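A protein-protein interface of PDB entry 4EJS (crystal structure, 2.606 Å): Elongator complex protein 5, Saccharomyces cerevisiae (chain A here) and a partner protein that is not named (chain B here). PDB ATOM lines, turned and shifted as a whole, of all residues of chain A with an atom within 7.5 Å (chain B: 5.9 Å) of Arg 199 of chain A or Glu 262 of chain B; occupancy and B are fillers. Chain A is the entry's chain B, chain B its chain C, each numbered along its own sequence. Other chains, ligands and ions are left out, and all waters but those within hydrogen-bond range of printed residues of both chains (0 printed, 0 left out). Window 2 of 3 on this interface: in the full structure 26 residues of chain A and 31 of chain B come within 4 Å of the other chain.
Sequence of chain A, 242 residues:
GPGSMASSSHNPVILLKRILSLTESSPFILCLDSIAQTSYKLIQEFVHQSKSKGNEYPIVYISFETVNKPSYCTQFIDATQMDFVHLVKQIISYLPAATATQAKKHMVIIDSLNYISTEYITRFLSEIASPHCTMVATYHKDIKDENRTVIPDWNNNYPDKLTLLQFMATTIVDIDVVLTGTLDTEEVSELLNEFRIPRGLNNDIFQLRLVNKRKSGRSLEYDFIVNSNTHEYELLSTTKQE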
ATOM      1  N   VAL A 177      16.109  21.491   1.939  1.00  0.00           N
ATOM      2  CA  VAL A 177      15.378  20.312   2.394  1.00  0.00           C
ATOM      3  C   VAL A 177      13.868  20.606   2.424  1.00  0.00           C
ATOM      4  O   VAL A 177      13.454  21.745   2.662  1.00  0.00           O
ATOM      5  CB  VAL A 177      15.872  19.903   3.805  1.00  0.00           C
ATOM      6  CG1 VAL A 177      15.529  20.974   4.807  1.00  0.00           C
ATOM      7  CG2 VAL A 177      15.282  18.578   4.234  1.00  0.00           C
ATOM      8  N   LEU A 179      10.697  19.843   4.694  1.00  0.00           N
ATOM      9  CA  LEU A 179      10.456  19.322   6.042  1.00  0.00           C
ATOM     10  C   LEU A 179       9.054  18.726   6.263  1.00  0.00           C
ATOM     11  O   LEU A 179       8.034  19.420   6.202  1.00  0.00           O
ATOM     12  CB  LEU A 179      10.755  20.398   7.087  1.00  0.00           C
ATOM     13  CG  LEU A 179      12.147  20.379   7.726  1.00  0.00           C
ATOM     14  CD1 LEU A 179      12.883  19.087   7.388  1.00  0.00           C
ATOM     15  CD2 LEU A 179      12.953  21.596   7.321  1.00  0.00           C
ATOM     16  N   THR A 180       9.033  17.425   6.528  1.00  0.00           N
ATOM     17  CA  THR A 180       7.806  16.658   6.725  1.00  0.00           C
ATOM     18  C   THR A 180       7.392  16.673   8.192  1.00  0.00           C
ATOM     19  O   THR A 180       6.248  16.373   8.528  1.00  0.00           O
ATOM     20  CB  THR A 180       8.004  15.186   6.269  1.00  0.00           C
ATOM     21  OG1 THR A 180       6.923  14.375   6.744  1.00  0.00           O
ATOM     22  CG2 THR A 180       9.332  14.622   6.800  1.00  0.00           C
ATOM     23  N   GLY A 181       8.332  17.023   9.064  1.00  0.00           N
ATOM     24  CA  GLY A 181       8.077  17.010  10.484  1.00  0.00           C
ATOM     25  C   GLY A 181       7.677  18.350  11.082  1.00  0.00           C
ATOM     26  O   GLY A 181       7.074  19.221  10.435  1.00  0.00           O
ATOM     27  N   LEU A 183       9.780  20.720  12.619  1.00  0.00           N
ATOM     28  CA  LEU A 183      10.707  21.836  12.424  1.00  0.00           C
ATOM     29  C   LEU A 183      10.671  22.438  11.030  1.00  0.00           C
ATOM     30  O   LEU A 183      10.439  21.735  10.056  1.00  0.00           O
ATOM     31  CB  LEU A 183      12.136  21.367  12.683  1.00  0.00           C
ATOM     32  CG  LEU A 183      12.390  20.628  13.992  1.00  0.00           C
ATOM     33  CD1 LEU A 183      13.806  20.092  14.019  1.00  0.00           C
ATOM     34  CD2 LEU A 183      12.128  21.537  15.176  1.00  0.00           C
ATOM     35  N   VAL A 188      16.286  24.091  11.747  1.00  0.00           N
ATOM     36  CA  VAL A 188      17.131  22.997  11.323  1.00  0.00           C
ATOM     37  C   VAL A 188      18.555  23.477  11.035  1.00  0.00           C
ATOM     38  O   VAL A 188      19.532  22.805  11.376  1.00  0.00           O
ATOM     39  CB  VAL A 188      16.518  22.295  10.096  1.00  0.00           C
ATOM     40  CG1 VAL A 188      17.499  21.332   9.473  1.00  0.00           C
ATOM     41  CG2 VAL A 188      15.250  21.575  10.508  1.00  0.00           C
ATOM     42  N   ARG A 196      23.935  18.796  15.270  1.00  0.00           N
ATOM     43  CA  ARG A 196      22.842  17.965  15.767  1.00  0.00           C
ATOM     44  C   ARG A 196      21.984  17.605  14.567  1.00  0.00           C
ATOM     45  O   ARG A 196      21.277  18.450  14.022  1.00  0.00           O
ATOM     46  CB  ARG A 196      22.020  18.737  16.780  1.00  0.00           C
ATOM     47  CG  ARG A 196      22.872  19.330  17.888  1.00  0.00           C
ATOM     48  CD  ARG A 196      22.038  19.663  19.115  1.00  0.00           C
ATOM     49  NE  ARG A 196      21.514  21.015  19.068  1.00  0.00           N
ATOM     50  CZ  ARG A 196      20.402  21.408  19.681  1.00  0.00           C
ATOM     51  NH1 ARG A 196      19.679  20.545  20.377  1.00  0.00           N
ATOM     52  NH2 ARG A 196      20.008  22.668  19.591  1.00  0.00           N
ATOM     53  N   ILE A 197      22.091  16.361  14.127  1.00  0.00           N
ATOM     54  CA  ILE A 197      21.443  15.931  12.903  1.00  0.00           C
ATOM     55  C   ILE A 197      20.104  15.325  13.262  1.00  0.00           C
ATOM     56  O   ILE A 197      20.047  14.316  13.960  1.00  0.00           O
ATOM     57  CB  ILE A 197      22.286  14.881  12.170  1.00  0.00           C
ATOM     58  CG1 ILE A 197      23.749  15.331  12.154  1.00  0.00           C
ATOM     59  CG2 ILE A 197      21.719  14.613  10.762  1.00  0.00           C
ATOM     60  CD1 ILE A 197      23.971  16.638  11.406  1.00  0.00           C
ATOM     61  N   PRO A 198      19.017  15.973  12.823  1.00  0.00           N
ATOM     62  CA  PRO A 198      17.676  15.415  13.015  1.00  0.00           C
ATOM     63  C   PRO A 198      17.361  14.378  11.930  1.00  0.00           C
ATOM     64  O   PRO A 198      18.084  14.246  10.929  1.00  0.00           O
ATOM     65  CB  PRO A 198      16.775  16.638  12.851  1.00  0.00           C
ATOM     66  CG  PRO A 198      17.525  17.485  11.830  1.00  0.00           C
ATOM     67  CD  PRO A 198      18.982  17.305  12.178  1.00  0.00           C
ATOM     68  N   ARG A 199      16.295  13.620  12.149  1.00  0.00           N
ATOM     69  CA  ARG A 199      15.859  12.659  11.162  1.00  0.00           C
ATOM     70  C   ARG A 199      15.143  13.443  10.055  1.00  0.00           C
ATOM     71  O   ARG A 199      14.884  14.631  10.211  1.00  0.00           O
ATOM     72  CB  ARG A 199      14.943  11.631  11.812  1.00  0.00           C
ATOM     73  CG  ARG A 199      13.652  12.218  12.356  1.00  0.00           C
ATOM     74  CD  ARG A 199      12.874  11.181  13.140  1.00  0.00           C
ATOM     75  NE  ARG A 199      12.639   9.982  12.342  1.00  0.00           N
ATOM     76  CZ  ARG A 199      12.530   8.757  12.846  1.00  0.00           C
ATOM     77  NH1 ARG A 199      12.643   8.564  14.158  1.00  0.00           N
ATOM     78  NH2 ARG A 199      12.313   7.727  12.036  1.00  0.00           N
ATOM     79  N   GLY A 200      14.857  12.798   8.928  1.00  0.00           N
ATOM     80  CA  GLY A 200      14.130  13.433   7.837  1.00  0.00           C
ATOM     81  C   GLY A 200      14.836  14.497   7.025  1.00  0.00           C
ATOM     82  O   GLY A 200      14.163  15.394   6.520  1.00  0.00           O
ATOM     83  N   LEU A 201      16.171  14.417   6.901  1.00  0.00           N
ATOM     84  CA  LEU A 201      16.885  15.232   5.913  1.00  0.00           C
ATOM     85  C   LEU A 201      17.233  14.381   4.695  1.00  0.00           C
ATOM     86  O   LEU A 201      17.055  13.160   4.711  1.00  0.00           O
ATOM     87  CB  LEU A 201      18.154  15.856   6.491  1.00  0.00           C
ATOM     88  CG  LEU A 201      18.070  16.569   7.840  1.00  0.00           C
ATOM     89  CD1 LEU A 201      19.452  17.038   8.241  1.00  0.00           C
ATOM     90  CD2 LEU A 201      17.100  17.728   7.801  1.00  0.00           C
ATOM     91  N   ASN A 202      17.719  15.026   3.638  1.00  0.00           N
ATOM     92  CA  ASN A 202      18.189  14.318   2.436  1.00  0.00           C
ATOM     93  C   ASN A 202      17.182  13.366   1.794  1.00  0.00           C
ATOM     94  O   ASN A 202      17.402  12.155   1.703  1.00  0.00           O
ATOM     95  CB  ASN A 202      19.498  13.593   2.721  1.00  0.00           C
ATOM     96  CG  ASN A 202      20.665  14.551   2.875  1.00  0.00           C
ATOM     97  OD1 ASN A 202      21.153  14.776   3.987  1.00  0.00           O
ATOM     98  ND2 ASN A 202      21.126  15.118   1.755  1.00  0.00           N
ATOM     99  N   ASN A 203      16.098  13.954   1.310  1.00  0.00           N
ATOM    100  CA  ASN A 203      14.921  13.228   0.865  1.00  0.00           C
ATOM    101  C   ASN A 203      14.878  13.137  -0.645  1.00  0.00           C
ATOM    102  O   ASN A 203      15.631  13.837  -1.317  1.00  0.00           O
ATOM    103  CB  ASN A 203      13.679  13.960   1.387  1.00  0.00           C
ATOM    104  CG  ASN A 203      13.638  14.004   2.904  1.00  0.00           C
ATOM    105  OD1 ASN A 203      13.676  12.961   3.555  1.00  0.00           O
ATOM    106  ND2 ASN A 203      13.605  15.211   3.475  1.00  0.00           N
ATOM    107  N   LEU B 240      21.649   7.089  20.710  1.00  0.00           N
ATOM    108  CA  LEU B 240      22.273   6.704  19.463  1.00  0.00           C
ATOM    109  C   LEU B 240      21.307   7.089  18.360  1.00  0.00           C
ATOM    110  O   LEU B 240      20.198   6.580  18.330  1.00  0.00           O
ATOM    111  CB  LEU B 240      22.462   5.196  19.442  1.00  0.00           C
ATOM    112  CG  LEU B 240      23.407   4.551  18.425  1.00  0.00           C
ATOM    113  CD1 LEU B 240      22.690   3.460  17.656  1.00  0.00           C
ATOM    114  CD2 LEU B 240      24.062   5.557  17.484  1.00  0.00           C
ATOM    115  N   HIS B 241      21.716   8.001  17.474  1.00  0.00           N
ATOM    116  CA  HIS B 241      20.895   8.399  16.336  1.00  0.00           C
ATOM    117  C   HIS B 241      21.461   7.786  15.080  1.00  0.00           C
ATOM    118  O   HIS B 241      22.665   7.854  14.849  1.00  0.00           O
ATOM    119  CB  HIS B 241      20.895   9.910  16.134  1.00  0.00           C
ATOM    120  CG  HIS B 241      20.316  10.681  17.270  1.00  0.00           C
ATOM    121  ND1 HIS B 241      19.402  10.144  18.148  1.00  0.00           N
ATOM    122  CD2 HIS B 241      20.525  11.952  17.680  1.00  0.00           C
ATOM    123  CE1 HIS B 241      19.074  11.048  19.050  1.00  0.00           C
ATOM    124  NE2 HIS B 241      19.739  12.158  18.786  1.00  0.00           N
ATOM    125  N   VAL B 242      20.580   7.194  14.275  1.00  0.00           N
ATOM    126  CA  VAL B 242      20.911   6.740  12.935  1.00  0.00           C
ATOM    127  C   VAL B 242      20.252   7.690  11.912  1.00  0.00           C
ATOM    128  O   VAL B 242      19.021   7.913  11.941  1.00  0.00           O
ATOM    129  CB  VAL B 242      20.395   5.313  12.730  1.00  0.00           C
ATOM    130  CG1 VAL B 242      20.814   4.745  11.350  1.00  0.00           C
ATOM    131  CG2 VAL B 242      20.848   4.430  13.877  1.00  0.00           C
ATOM    132  N   CYS B 243      21.076   8.243  11.021  1.00  0.00           N
ATOM    133  CA  CYS B 243      20.645   9.217  10.014  1.00  0.00           C
ATOM    134  C   CYS B 243      21.195   8.871   8.639  1.00  0.00           C
ATOM    135  O   CYS B 243      22.214   8.199   8.524  1.00  0.00           O
ATOM    136  CB  CYS B 243      21.159  10.619  10.367  1.00  0.00           C
ATOM    137  SG  CYS B 243      20.866  11.161  12.059  1.00  0.00           S
ATOM    138  N   ARG B 244      20.526   9.349   7.595  1.00  0.00           N
ATOM    139  CA  ARG B 244      21.095   9.330   6.254  1.00  0.00           C
ATOM    140  C   ARG B 244      22.295  10.263   6.246  1.00  0.00           C
ATOM    141  O   ARG B 244      22.301  11.287   6.938  1.00  0.00           O
ATOM    142  CB  ARG B 244      20.086   9.838   5.219  1.00  0.00           C
ATOM    143  CG  ARG B 244      19.179   8.808   4.638  1.00  0.00           C
ATOM    144  CD  ARG B 244      18.199   9.404   3.616  1.00  0.00           C
ATOM    145  NE  ARG B 244      17.242  10.339   4.222  1.00  0.00           N
ATOM    146  CZ  ARG B 244      16.212   9.972   4.980  1.00  0.00           C
ATOM    147  NH1 ARG B 244      16.015   8.685   5.249  1.00  0.00           N
ATOM    148  NH2 ARG B 244      15.397  10.889   5.490  1.00  0.00           N
ATOM    149  N   GLU B 260      16.416   5.255   9.582  1.00  0.00           N
ATOM    150  CA  GLU B 260      16.636   6.284  10.576  1.00  0.00           C
ATOM    151  C   GLU B 260      15.952   5.913  11.874  1.00  0.00           C
ATOM    152  O   GLU B 260      14.869   5.333  11.872  1.00  0.00           O
ATOM    153  CB  GLU B 260      16.193   7.659  10.056  1.00  0.00           C
ATOM    154  CG  GLU B 260      17.018   8.162   8.826  1.00  0.00           C
ATOM    155  CD  GLU B 260      16.978   9.690   8.657  1.00  0.00           C
ATOM    156  OE1 GLU B 260      15.865  10.267   8.729  1.00  0.00           O
ATOM    157  OE2 GLU B 260      18.056  10.318   8.472  1.00  0.00           O
ATOM    158  N   ASN B 261      16.602   6.245  12.985  1.00  0.00           N
ATOM    159  CA  ASN B 261      16.195   5.757  14.287  1.00  0.00           C
ATOM    160  C   ASN B 261      16.868   6.518  15.408  1.00  0.00           C
ATOM    161  O   ASN B 261      17.939   7.106  15.205  1.00  0.00           O
ATOM    162  CB  ASN B 261      16.593   4.288  14.394  1.00  0.00           C
ATOM    163  CG  ASN B 261      15.447   3.407  14.798  1.00  0.00           C
ATOM    164  OD1 ASN B 261      14.672   3.754  15.686  1.00  0.00           O
ATOM    165  ND2 ASN B 261      15.327   2.257  14.144  1.00  0.00           N
ATOM    166  N   GLU B 262      16.238   6.508  16.583  1.00  0.00           N
ATOM    167  CA  GLU B 262      16.861   6.945  17.842  1.00  0.00           C
ATOM    168  C   GLU B 262      16.717   5.827  18.866  1.00  0.00           C
ATOM    169  O   GLU B 262      15.626   5.293  19.058  1.00  0.00           O
ATOM    170  CB  GLU B 262      16.208   8.214  18.410  1.00  0.00           C
ATOM    171  CG  GLU B 262      16.220   9.419  17.487  1.00  0.00           C
ATOM    172  CD  GLU B 262      14.965   9.529  16.640  1.00  0.00           C
ATOM    173  OE1 GLU B 262      13.914   8.991  17.058  1.00  0.00           O
ATOM    174  OE2 GLU B 262      15.028  10.149  15.555  1.00  0.00           O
ATOM    175  N   TYR B 263      17.818   5.476  19.514  1.00  0.00           N
ATOM    176  CA  TYR B 263      17.801   4.482  20.570  1.00  0.00           C
ATOM    177  C   TYR B 263      18.300   5.170  21.820  1.00  0.00           C
ATOM    178  O   TYR B 263      18.937   6.217  21.731  1.00  0.00           O
ATOM    179  CB  TYR B 263      18.772   3.338  20.253  1.00  0.00           C
ATOM    180  CG  TYR B 263      18.460   2.491  19.031  1.00  0.00           C
ATOM    181  CD1 TYR B 263      17.697   1.333  19.145  1.00  0.00           C
ATOM    182  CD2 TYR B 263      18.969   2.822  17.769  1.00  0.00           C
ATOM    183  CE1 TYR B 263      17.424   0.537  18.044  1.00  0.00           C
ATOM    184  CE2 TYR B 263      18.695   2.027  16.650  1.00  0.00           C
ATOM    185  CZ  TYR B 263      17.919   0.883  16.801  1.00  0.00           C
ATOM    186  OH  TYR B 263      17.626   0.072  15.722  1.00  0.00           O
ATOM    187  N   LEU B 264      18.005   4.591  22.981  1.00  0.00           N
ATOM    188  CA  LEU B 264      18.753   4.887  24.202  1.00  0.00           C
ATOM    189  C   LEU B 264      19.637   3.682  24.392  1.00  0.00           C
ATOM    190  O   LEU B 264      19.282   2.582  23.970  1.00  0.00           O
ATOM    191  CB  LEU B 264      17.850   5.027  25.426  1.00  0.00           C
ATOM    192  CG  LEU B 264      16.886   6.207  25.461  1.00  0.00           C
ATOM    193  CD1 LEU B 264      16.165   6.267  26.796  1.00  0.00           C
ATOM    194  CD2 LEU B 264      17.647   7.489  25.202  1.00  0.00           C
ATOM    195  N   PHE B 275      17.644   0.285  23.754  1.00  0.00           N
ATOM    196  CA  PHE B 275      16.226   0.284  24.102  1.00  0.00           C
ATOM    197  C   PHE B 275      15.537   1.594  23.733  1.00  0.00           C
ATOM    198  O   PHE B 275      16.104   2.671  23.891  1.00  0.00           O
ATOM    199  CB  PHE B 275      16.023  -0.069  25.588  1.00  0.00           C
ATOM    200  CG  PHE B 275      16.785   0.818  26.558  1.00  0.00           C
ATOM    201  CD1 PHE B 275      16.137   1.830  27.260  1.00  0.00           C
ATOM    202  CD2 PHE B 275      18.142   0.620  26.794  1.00  0.00           C
ATOM    203  CE1 PHE B 275      16.833   2.638  28.167  1.00  0.00           C
ATOM    204  CE2 PHE B 275      18.851   1.431  27.696  1.00  0.00           C
ATOM    205  CZ  PHE B 275      18.198   2.437  28.383  1.00  0.00           C
ATOM    206  N   TYR B 276      14.315   1.495  23.221  1.00  0.00           N
ATOM    207  CA  TYR B 276      13.507   2.680  22.931  1.00  0.00           C
ATOM    208  C   TYR B 276      12.912   3.272  24.210  1.00  0.00           C
ATOM    209  O   TYR B 276      12.547   4.451  24.253  1.00  0.00           O
ATOM    210  CB  TYR B 276      12.367   2.336  21.977  1.00  0.00           C
ATOM    211  CG  TYR B 276      12.808   1.744  20.666  1.00  0.00           C
ATOM    212  CD1 TYR B 276      12.130   0.664  20.117  1.00  0.00           C
ATOM    213  CD2 TYR B 276      13.890   2.264  19.970  1.00  0.00           C
ATOM    214  CE1 TYR B 276      12.519   0.109  18.912  1.00  0.00           C
ATOM    215  CE2 TYR B 276      14.286   1.715  18.759  1.00  0.00           C
ATOM    216  CZ  TYR B 276      13.595   0.636  18.236  1.00  0.00           C
ATOM    217  OH  TYR B 276      13.965   0.073  17.035  1.00  0.00           O
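The side-chain carboxylate (OE2) of Glu 262 of chain B is in salt-bridge range of the guanidinium group (NH1) of Arg 199 of chain A, 3.2 Å away. The backbone NH (N) of Gly 200 of chain A sits at hydrogen-bond distance from the side-chain carboxylate (OE1) of Glu 260 of chain B, 2.7 Å away. The backbone carbonyl oxygen (O) of Leu 201 of chain A sits at hydrogen-bond distance from the guanidinium group (NE) of Arg 244 of chain B (2.9 Å). NE of Arg 244 of chain B sits at hydrogen-bond distance from O of Asn 202 of chain A. NH2 of Arg 244 of chain B lies within hydrogen-bond range of OD1 of Asn 203 of chain A (3.3 Å). O of Ile 197 of chain A sits at hydrogen-bond distance from SG of Cys 243 of chain B.
Of the 14 printed residues of chain A, 6 touch a printed residue of chain B. Hydrophobic or aromatic side chains of chain A within 4 Å of the printed part of chain B: Ile 197. Along chain A the printed residues that touch a printed residue of chain B span positions 197 to 203.
The guanidinium group (NH2) of Arg 244 of chain B is in salt-bridge range of the side-chain carboxylate (OE1) of Glu 260 of chain B. The backbone carbonyl oxygen of Gly 200 of chain A is in hydrogen-bond range of the side-chain amide nitrogen of Asn 203 of chain A (3.1 Å).
Of chain B, only Glu 260 (3.4 Å) and Glu 262 (3.2 Å) come within 4 Å of Arg 199 of chain A. Glu 262 of chain B touches one residue of chain A. Of the printed residues of chain A, Arg 244 of chain B touches Gly 200 (3.7 Å), Leu 201 (2.9 Å), Asn 202 (3.1 Å) and Asn 203 (3.3 Å). Of the printed residues of chain B, Asn 202 of chain A touches Arg 244. Printed residues of chain B within 4 Å of Leu 201 of chain A: Arg 244. Leu 179 of chain A touches none of the printed residues of chain B. The nearest printed residue of chain A that does not touch Cys 243 of chain B is Pro 198 of chain A (4.3 Å).
Among the printed residues, pairs that only touch across the chains: Arg 199 of chain A with Glu 260 of chain B and Gly 200 of chain A with Arg 244 of chain B.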
